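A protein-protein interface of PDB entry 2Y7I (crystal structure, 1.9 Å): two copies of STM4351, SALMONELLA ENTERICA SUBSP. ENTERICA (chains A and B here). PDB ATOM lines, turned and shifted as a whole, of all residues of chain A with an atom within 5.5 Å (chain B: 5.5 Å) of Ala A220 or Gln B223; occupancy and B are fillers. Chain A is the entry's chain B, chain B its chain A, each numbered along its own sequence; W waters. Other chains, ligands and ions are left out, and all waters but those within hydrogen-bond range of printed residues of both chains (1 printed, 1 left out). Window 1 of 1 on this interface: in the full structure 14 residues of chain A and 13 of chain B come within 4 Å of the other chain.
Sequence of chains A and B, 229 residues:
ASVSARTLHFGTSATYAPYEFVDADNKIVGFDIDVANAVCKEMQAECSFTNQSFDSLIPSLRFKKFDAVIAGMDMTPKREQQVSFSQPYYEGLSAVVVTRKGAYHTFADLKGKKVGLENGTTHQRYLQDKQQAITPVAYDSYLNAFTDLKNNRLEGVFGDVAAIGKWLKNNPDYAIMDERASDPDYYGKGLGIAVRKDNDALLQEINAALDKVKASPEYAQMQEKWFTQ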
ATOM      1  N   LYS A 214      31.048  26.315  -3.599  1.00  0.00           N
ATOM      2  CA  LYS A 214      31.109  25.026  -4.289  1.00  0.00           C
ATOM      3  C   LYS A 214      29.924  24.126  -3.941  1.00  0.00           C
ATOM      4  O   LYS A 214      29.656  23.154  -4.638  1.00  0.00           O
ATOM      5  CB  LYS A 214      32.443  24.319  -4.018  1.00  0.00           C
ATOM      6  CG  LYS A 214      33.666  25.024  -4.637  1.00  0.00           C
ATOM      7  CD  LYS A 214      34.972  24.562  -3.992  1.00  0.00           C
ATOM      8  CE  LYS A 214      35.188  23.064  -4.160  1.00  0.00           C
ATOM      9  NZ  LYS A 214      36.396  22.597  -3.434  1.00  0.00           N
ATOM     10  N   ALA A 215      29.208  24.460  -2.872  1.00  0.00           N
ATOM     11  CA  ALA A 215      28.008  23.708  -2.513  1.00  0.00           C
ATOM     12  C   ALA A 215      26.763  24.273  -3.201  1.00  0.00           C
ATOM     13  O   ALA A 215      25.671  23.742  -3.035  1.00  0.00           O
ATOM     14  CB  ALA A 215      27.818  23.688  -0.989  1.00  0.00           C
ATOM     15  N   SER A 216      26.934  25.347  -3.971  1.00  0.00           N
ATOM     16  CA  SER A 216      25.787  26.079  -4.527  1.00  0.00           C
ATOM     17  C   SER A 216      25.398  25.595  -5.924  1.00  0.00           C
ATOM     18  O   SER A 216      26.261  25.214  -6.700  1.00  0.00           O
ATOM     19  CB  SER A 216      26.065  27.593  -4.543  1.00  0.00           C
ATOM     20  OG  SER A 216      27.028  27.957  -5.523  1.00  0.00           O
ATOM     21  N   PRO A 217      24.087  25.605  -6.242  1.00  0.00           N
ATOM     22  CA  PRO A 217      23.676  25.318  -7.620  1.00  0.00           C
ATOM     23  C   PRO A 217      24.262  26.309  -8.624  1.00  0.00           C
ATOM     24  O   PRO A 217      24.515  25.925  -9.768  1.00  0.00           O
ATOM     25  CB  PRO A 217      22.140  25.419  -7.577  1.00  0.00           C
ATOM     26  CG  PRO A 217      21.787  25.943  -6.242  1.00  0.00           C
ATOM     27  CD  PRO A 217      22.936  25.661  -5.326  1.00  0.00           C
ATOM     28  N   GLU A 218      24.502  27.552  -8.190  1.00  0.00           N
ATOM     29  CA  GLU A 218      25.136  28.599  -9.023  1.00  0.00           C
ATOM     30  C   GLU A 218      26.504  28.198  -9.562  1.00  0.00           C
ATOM     31  O   GLU A 218      26.859  28.540 -10.683  1.00  0.00           O
ATOM     32  CB  GLU A 218      25.303  29.916  -8.256  1.00  0.00           C
ATOM     33  CG  GLU A 218      24.008  30.694  -8.020  1.00  0.00           C
ATOM     34  CD  GLU A 218      23.150  30.085  -6.926  1.00  0.00           C
ATOM     35  OE1 GLU A 218      23.688  29.324  -6.093  1.00  0.00           O
ATOM     36  OE2 GLU A 218      21.926  30.357  -6.895  1.00  0.00           O
ATOM     37  N   TYR A 219      27.273  27.490  -8.747  1.00  0.00           N
ATOM     38  CA  TYR A 219      28.614  27.073  -9.134  1.00  0.00           C
ATOM     39  C   TYR A 219      28.581  25.985 -10.226  1.00  0.00           C
ATOM     40  O   TYR A 219      29.425  25.979 -11.126  1.00  0.00           O
ATOM     41  CB  TYR A 219      29.372  26.646  -7.876  1.00  0.00           C
ATOM     42  CG  TYR A 219      30.691  25.951  -8.052  1.00  0.00           C
ATOM     43  CD1 TYR A 219      31.834  26.636  -8.488  1.00  0.00           C
ATOM     44  CD2 TYR A 219      30.815  24.615  -7.715  1.00  0.00           C
ATOM     45  CE1 TYR A 219      33.065  25.963  -8.615  1.00  0.00           C
ATOM     46  CE2 TYR A 219      32.013  23.950  -7.830  1.00  0.00           C
ATOM     47  CZ  TYR A 219      33.131  24.617  -8.275  1.00  0.00           C
ATOM     48  OH  TYR A 219      34.304  23.894  -8.371  1.00  0.00           O
ATOM     49  N   ALA A 220      27.605  25.080 -10.144  1.00  0.00           N
ATOM     50  CA  ALA A 220      27.371  24.101 -11.205  1.00  0.00           C
ATOM     51  C   ALA A 220      27.001  24.809 -12.513  1.00  0.00           C
ATOM     52  O   ALA A 220      27.501  24.449 -13.586  1.00  0.00           O
ATOM     53  CB  ALA A 220      26.276  23.107 -10.804  1.00  0.00           C
ATOM     54  N   GLN A 221      26.142  25.826 -12.406  1.00  0.00           N
ATOM     55  CA  GLN A 221      25.740  26.638 -13.559  1.00  0.00           C
ATOM     56  C   GLN A 221      26.934  27.362 -14.180  1.00  0.00           C
ATOM     57  O   GLN A 221      27.010  27.475 -15.406  1.00  0.00           O
ATOM     58  CB  GLN A 221      24.635  27.640 -13.182  1.00  0.00           C
ATOM     59  CG  GLN A 221      23.314  26.994 -12.762  1.00  0.00           C
ATOM     60  CD  GLN A 221      22.293  28.001 -12.246  1.00  0.00           C
ATOM     61  OE1 GLN A 221      22.647  29.026 -11.656  1.00  0.00           O
ATOM     62  NE2 GLN A 221      21.014  27.711 -12.470  1.00  0.00           N
ATOM     63  N   MET A 222      27.863  27.837 -13.340  1.00  0.00           N
ATOM     64  CA  MET A 222      29.107  28.453 -13.827  1.00  0.00           C
ATOM     65  C   MET A 222      29.898  27.514 -14.739  1.00  0.00           C
ATOM     66  O   MET A 222      30.347  27.917 -15.805  1.00  0.00           O
ATOM     67  CB  MET A 222      30.018  28.894 -12.678  1.00  0.00           C
ATOM     68  CG  MET A 222      29.554  30.096 -11.899  1.00  0.00           C
ATOM     69  SD  MET A 222      30.710  30.460 -10.561  1.00  0.00           S
ATOM     70  CE  MET A 222      29.580  31.281  -9.457  1.00  0.00           C
ATOM     71  N   GLN A 223      30.058  26.264 -14.312  1.00  0.00           N
ATOM     72  CA  GLN A 223      30.763  25.269 -15.105  1.00  0.00           C
ATOM     73  C   GLN A 223      30.016  24.981 -16.400  1.00  0.00           C
ATOM     74  O   GLN A 223      30.630  24.844 -17.464  1.00  0.00           O
ATOM     75  CB  GLN A 223      30.933  23.983 -14.306  1.00  0.00           C
ATOM     76  CG  GLN A 223      31.792  24.140 -13.072  1.00  0.00           C
ATOM     77  CD  GLN A 223      31.825  22.883 -12.240  1.00  0.00           C
ATOM     78  OE1 GLN A 223      31.608  22.929 -11.028  1.00  0.00           O
ATOM     79  NE2 GLN A 223      32.089  21.747 -12.883  1.00  0.00           N
ATOM     80  N   GLU A 224      28.691  24.906 -16.307  1.00  0.00           N
ATOM     81  CA  GLU A 224      27.862  24.672 -17.474  1.00  0.00           C
ATOM     82  C   GLU A 224      27.967  25.861 -18.450  1.00  0.00           C
ATOM     83  O   GLU A 224      27.943  25.678 -19.669  1.00  0.00           O
ATOM     84  CB  GLU A 224      26.413  24.337 -17.059  1.00  0.00           C
ATOM     85  CG  GLU A 224      26.298  22.940 -16.351  1.00  0.00           C
ATOM     86  CD  GLU A 224      24.996  22.698 -15.555  1.00  0.00           C
ATOM     87  OE1 GLU A 224      24.223  23.655 -15.307  1.00  0.00           O
ATOM     88  OE2 GLU A 224      24.752  21.527 -15.167  1.00  0.00           O
ATOM     89  N   LYS A 225      28.128  27.070 -17.914  1.00  0.00           N
ATOM     90  CA  LYS A 225      28.293  28.250 -18.756  1.00  0.00           C
ATOM     91  C   LYS A 225      29.637  28.244 -19.480  1.00  0.00           C
ATOM     92  O   LYS A 225      29.695  28.436 -20.699  1.00  0.00           O
ATOM     93  CB  LYS A 225      28.125  29.541 -17.953  1.00  0.00           C
ATOM     94  CG  LYS A 225      28.278  30.801 -18.802  1.00  0.00           C
ATOM     95  CD  LYS A 225      28.009  32.053 -18.006  1.00  0.00           C
ATOM     96  CE  LYS A 225      28.189  33.276 -18.887  1.00  0.00           C
ATOM     97  NZ  LYS A 225      27.610  34.487 -18.270  1.00  0.00           N
ATOM     98  N   PHE B  31      20.990  11.239  -4.824  1.00  0.00           N
ATOM     99  CA  PHE B  31      22.038  12.248  -4.792  1.00  0.00           C
ATOM    100  C   PHE B  31      23.027  11.986  -3.660  1.00  0.00           C
ATOM    101  O   PHE B  31      24.240  11.960  -3.892  1.00  0.00           O
ATOM    102  CB  PHE B  31      21.445  13.643  -4.664  1.00  0.00           C
ATOM    103  CG  PHE B  31      22.480  14.732  -4.588  1.00  0.00           C
ATOM    104  CD1 PHE B  31      23.173  15.132  -5.723  1.00  0.00           C
ATOM    105  CD2 PHE B  31      22.743  15.367  -3.378  1.00  0.00           C
ATOM    106  CE1 PHE B  31      24.124  16.158  -5.657  1.00  0.00           C
ATOM    107  CE2 PHE B  31      23.685  16.394  -3.301  1.00  0.00           C
ATOM    108  CZ  PHE B  31      24.379  16.775  -4.441  1.00  0.00           C
ATOM    109  N   TYR B  90      25.781  20.536  -0.066  1.00  0.00           N
ATOM    110  CA  TYR B  90      24.705  21.043  -0.913  1.00  0.00           C
ATOM    111  C   TYR B  90      23.896  22.038  -0.088  1.00  0.00           C
ATOM    112  O   TYR B  90      23.930  21.982   1.140  1.00  0.00           O
ATOM    113  CB  TYR B  90      23.805  19.900  -1.409  1.00  0.00           C
ATOM    114  CG  TYR B  90      22.846  20.301  -2.513  1.00  0.00           C
ATOM    115  CD1 TYR B  90      23.312  20.626  -3.789  1.00  0.00           C
ATOM    116  CD2 TYR B  90      21.473  20.356  -2.279  1.00  0.00           C
ATOM    117  CE1 TYR B  90      22.424  20.994  -4.809  1.00  0.00           C
ATOM    118  CE2 TYR B  90      20.585  20.715  -3.280  1.00  0.00           C
ATOM    119  CZ  TYR B  90      21.063  21.026  -4.539  1.00  0.00           C
ATOM    120  OH  TYR B  90      20.171  21.387  -5.522  1.00  0.00           O
ATOM    121  N   GLU B 218      32.102  15.867 -12.192  1.00  0.00           N
ATOM    122  CA  GLU B 218      31.148  14.814 -11.798  1.00  0.00           C
ATOM    123  C   GLU B 218      30.117  15.265 -10.776  1.00  0.00           C
ATOM    124  O   GLU B 218      28.972  14.807 -10.792  1.00  0.00           O
ATOM    125  CB  GLU B 218      31.882  13.584 -11.247  1.00  0.00           C
ATOM    126  CG  GLU B 218      32.640  12.771 -12.297  1.00  0.00           C
ATOM    127  CD  GLU B 218      34.063  13.273 -12.549  1.00  0.00           C
ATOM    128  OE1 GLU B 218      34.453  14.324 -11.997  1.00  0.00           O
ATOM    129  OE2 GLU B 218      34.799  12.613 -13.310  1.00  0.00           O
ATOM    130  N   TYR B 219      30.522  16.171  -9.894  1.00  0.00           N
ATOM    131  CA  TYR B 219      29.646  16.657  -8.841  1.00  0.00           C
ATOM    132  C   TYR B 219      28.582  17.588  -9.427  1.00  0.00           C
ATOM    133  O   TYR B 219      27.431  17.560  -9.001  1.00  0.00           O
ATOM    134  CB  TYR B 219      30.494  17.299  -7.739  1.00  0.00           C
ATOM    135  CG  TYR B 219      29.756  18.057  -6.669  1.00  0.00           C
ATOM    136  CD1 TYR B 219      28.992  17.401  -5.699  1.00  0.00           C
ATOM    137  CD2 TYR B 219      29.852  19.442  -6.607  1.00  0.00           C
ATOM    138  CE1 TYR B 219      28.327  18.126  -4.712  1.00  0.00           C
ATOM    139  CE2 TYR B 219      29.208  20.161  -5.641  1.00  0.00           C
ATOM    140  CZ  TYR B 219      28.447  19.510  -4.697  1.00  0.00           C
ATOM    141  OH  TYR B 219      27.815  20.277  -3.751  1.00  0.00           O
ATOM    142  N   ALA B 220      28.956  18.361 -10.449  1.00  0.00           N
ATOM    143  CA  ALA B 220      27.988  19.167 -11.202  1.00  0.00           C
ATOM    144  C   ALA B 220      26.998  18.252 -11.933  1.00  0.00           C
ATOM    145  O   ALA B 220      25.793  18.524 -11.970  1.00  0.00           O
ATOM    146  CB  ALA B 220      28.694  20.094 -12.175  1.00  0.00           C
ATOM    147  N   GLN B 221      27.514  17.154 -12.488  1.00  0.00           N
ATOM    148  CA  GLN B 221      26.673  16.166 -13.173  1.00  0.00           C
ATOM    149  C   GLN B 221      25.709  15.437 -12.225  1.00  0.00           C
ATOM    150  O   GLN B 221      24.585  15.125 -12.617  1.00  0.00           O
ATOM    151  CB  GLN B 221      27.531  15.170 -13.964  1.00  0.00           C
ATOM    152  CG  GLN B 221      28.342  15.813 -15.088  1.00  0.00           C
ATOM    153  CD  GLN B 221      29.542  14.975 -15.509  1.00  0.00           C
ATOM    154  OE1 GLN B 221      29.785  13.888 -14.970  1.00  0.00           O
ATOM    155  NE2 GLN B 221      30.309  15.485 -16.471  1.00  0.00           N
ATOM    156  N   MET B 222      26.136  15.181 -10.984  1.00  0.00           N
ATOM    157  CA  MET B 222      25.247  14.591  -9.960  1.00  0.00           C
ATOM    158  C   MET B 222      24.034  15.478  -9.684  1.00  0.00           C
ATOM    159  O   MET B 222      22.911  14.987  -9.544  1.00  0.00           O
ATOM    160  CB  MET B 222      25.994  14.356  -8.646  1.00  0.00           C
ATOM    161  CG  MET B 222      26.992  13.219  -8.663  1.00  0.00           C
ATOM    162  SD  MET B 222      27.871  13.189  -7.086  1.00  0.00           S
ATOM    163  CE  MET B 222      29.236  12.104  -7.473  1.00  0.00           C
ATOM    164  N   GLN B 223      24.273  16.786  -9.601  1.00  0.00           N
ATOM    165  CA  GLN B 223      23.215  17.764  -9.366  1.00  0.00           C
ATOM    166  C   GLN B 223      22.259  17.828 -10.557  1.00  0.00           C
ATOM    167  O   GLN B 223      21.035  17.830 -10.382  1.00  0.00           O
ATOM    168  CB  GLN B 223      23.825  19.141  -9.096  1.00  0.00           C
ATOM    169  CG  GLN B 223      24.566  19.243  -7.751  1.00  0.00           C
ATOM    170  CD  GLN B 223      25.195  20.617  -7.524  1.00  0.00           C
ATOM    171  OE1 GLN B 223      26.373  20.727  -7.170  1.00  0.00           O
ATOM    172  NE2 GLN B 223      24.418  21.668  -7.749  1.00  0.00           N
ATOM    173  N   GLU B 224      22.830  17.881 -11.761  1.00  0.00           N
ATOM    174  CA  GLU B 224      22.073  17.801 -13.010  1.00  0.00           C
ATOM    175  C   GLU B 224      21.186  16.551 -13.056  1.00  0.00           C
ATOM    176  O   GLU B 224      20.002  16.637 -13.387  1.00  0.00           O
ATOM    177  CB  GLU B 224      23.039  17.838 -14.198  1.00  0.00           C
ATOM    178  CG  GLU B 224      22.437  17.549 -15.570  1.00  0.00           C
ATOM    179  CD  GLU B 224      23.488  17.542 -16.677  1.00  0.00           C
ATOM    180  OE1 GLU B 224      24.645  17.126 -16.430  1.00  0.00           O
ATOM    181  OE2 GLU B 224      23.152  17.951 -17.803  1.00  0.00           O
ATOM    182  N   LYS B 225      21.752  15.399 -12.708  1.00  0.00           N
ATOM    183  CA  LYS B 225      20.995  14.148 -12.734  1.00  0.00           C
ATOM    184  C   LYS B 225      19.812  14.155 -11.768  1.00  0.00           C
ATOM    185  O   LYS B 225      18.688  13.810 -12.148  1.00  0.00           O
ATOM    186  CB  LYS B 225      21.898  12.954 -12.421  1.00  0.00           C
ATOM    187  CG  LYS B 225      21.111  11.667 -12.184  1.00  0.00           C
ATOM    188  CD  LYS B 225      21.986  10.446 -12.156  1.00  0.00           C
ATOM    189  CE  LYS B 225      21.115   9.203 -12.205  1.00  0.00           C
ATOM    190  NZ  LYS B 225      21.934   7.966 -12.319  1.00  0.00           N
ATOM    191  N   TRP B 226      20.075  14.546 -10.522  1.00  0.00           N
ATOM    192  CA  TRP B 226      19.120  14.340  -9.446  1.00  0.00           C
ATOM    193  C   TRP B 226      18.170  15.507  -9.175  1.00  0.00           C
ATOM    194  O   TRP B 226      17.087  15.301  -8.624  1.00  0.00           O
ATOM    195  CB  TRP B 226      19.858  13.934  -8.160  1.00  0.00           C
ATOM    196  CG  TRP B 226      20.502  12.570  -8.236  1.00  0.00           C
ATOM    197  CD1 TRP B 226      21.848  12.292  -8.263  1.00  0.00           C
ATOM    198  CD2 TRP B 226      19.831  11.305  -8.305  1.00  0.00           C
ATOM    199  NE1 TRP B 226      22.052  10.928  -8.328  1.00  0.00           N
ATOM    200  CE2 TRP B 226      20.830  10.300  -8.356  1.00  0.00           C
ATOM    201  CE3 TRP B 226      18.480  10.921  -8.330  1.00  0.00           C
ATOM    202  CZ2 TRP B 226      20.520   8.936  -8.430  1.00  0.00           C
ATOM    203  CZ3 TRP B 226      18.174   9.566  -8.403  1.00  0.00           C
ATOM    204  CH2 TRP B 226      19.188   8.590  -8.453  1.00  0.00           C
ATOM    205  N   PHE B 227      18.559  16.718  -9.574  1.00  0.00           N
ATOM    206  CA  PHE B 227      17.781  17.917  -9.229  1.00  0.00           C
ATOM    207  C   PHE B 227      17.083  18.636 -10.398  1.00  0.00           C
ATOM    208  O   PHE B 227      16.336  19.589 -10.175  1.00  0.00           O
ATOM    209  CB  PHE B 227      18.624  18.893  -8.385  1.00  0.00           C
ATOM    210  CG  PHE B 227      19.017  18.343  -7.036  1.00  0.00           C
ATOM    211  CD1 PHE B 227      18.056  18.110  -6.055  1.00  0.00           C
ATOM    212  CD2 PHE B 227      20.341  18.052  -6.744  1.00  0.00           C
ATOM    213  CE1 PHE B 227      18.415  17.583  -4.813  1.00  0.00           C
ATOM    214  CE2 PHE B 227      20.704  17.538  -5.495  1.00  0.00           C
ATOM    215  CZ  PHE B 227      19.743  17.300  -4.533  1.00  0.00           C
ATOM    216  N   THR B 228      17.300  18.171 -11.629  1.00  0.00           N
ATOM    217  CA  THR B 228      16.619  18.739 -12.811  1.00  0.00           C
ATOM    218  C   THR B 228      15.197  18.195 -12.992  1.00  0.00           C
ATOM    219  O   THR B 228      14.558  17.732 -12.042  1.00  0.00           O
ATOM    220  CB  THR B 228      17.429  18.491 -14.108  1.00  0.00           C
ATOM    221  OG1 THR B 228      18.770  18.959 -13.928  1.00  0.00           O
ATOM    222  CG2 THR B 228      16.803  19.207 -15.318  1.00  0.00           C
HETATM  223  O   HOH W   1      28.930  21.801  -9.083  1.00  0.00           O
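CE2 of Tyr B219 touches O of Lys A214 (3.2 Å). Ala A215 touches Tyr B90. CA of Ala A215 touches OH of Tyr B219, 3.7 Å away. Pro A217 touches Gln B223. CB of Ala A220 touches NE2 of Gln B223, at 3.9 Å. NE2 of Gln A223 touches CB of Ala B220, 3.8 Å away.
Of the printed residues of chain B, Lys A214 touches Tyr B219 (3.2 Å). Printed residues of chain B within 4 Å of Ala A215: Tyr B90 and Tyr B219. Ala A220 touches one residue of chain B. Printed residues of chain A within 4 Å of Ala B220: Gln A223. Gln B223 touches just these residues of chain A: Pro A217 (3.7 Å) and Ala A220 (3.9 Å). The nearest printed residue of chain A that does not touch Ala B220 is Ala A220 (4.1 Å).
Of the 13 printed residues of chain B, 4 touch a printed residue of chain A. Printed residues of chain B that touch a printed residue of chain A: Tyr B90, Tyr B219, Ala B220 and Gln B223. Hydrophobic or aromatic side chains of chain A within 4 Å of the printed part of chain B: Ala A215 and Ala A220. Among the printed residues, no Asp or Glu carboxylate lies within 4 Å of a Lys or Arg side-chain nitrogen of the other chain.
Ala A220 touches Gln B223, and with the chains exchanged Gln A223 touches Ala B220.
Water W1 lies within hydrogen-bond range of the side-chain amide oxygen (OE1) of Gln B223 and the side-chain amide oxygen (OE1) of Gln A223.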
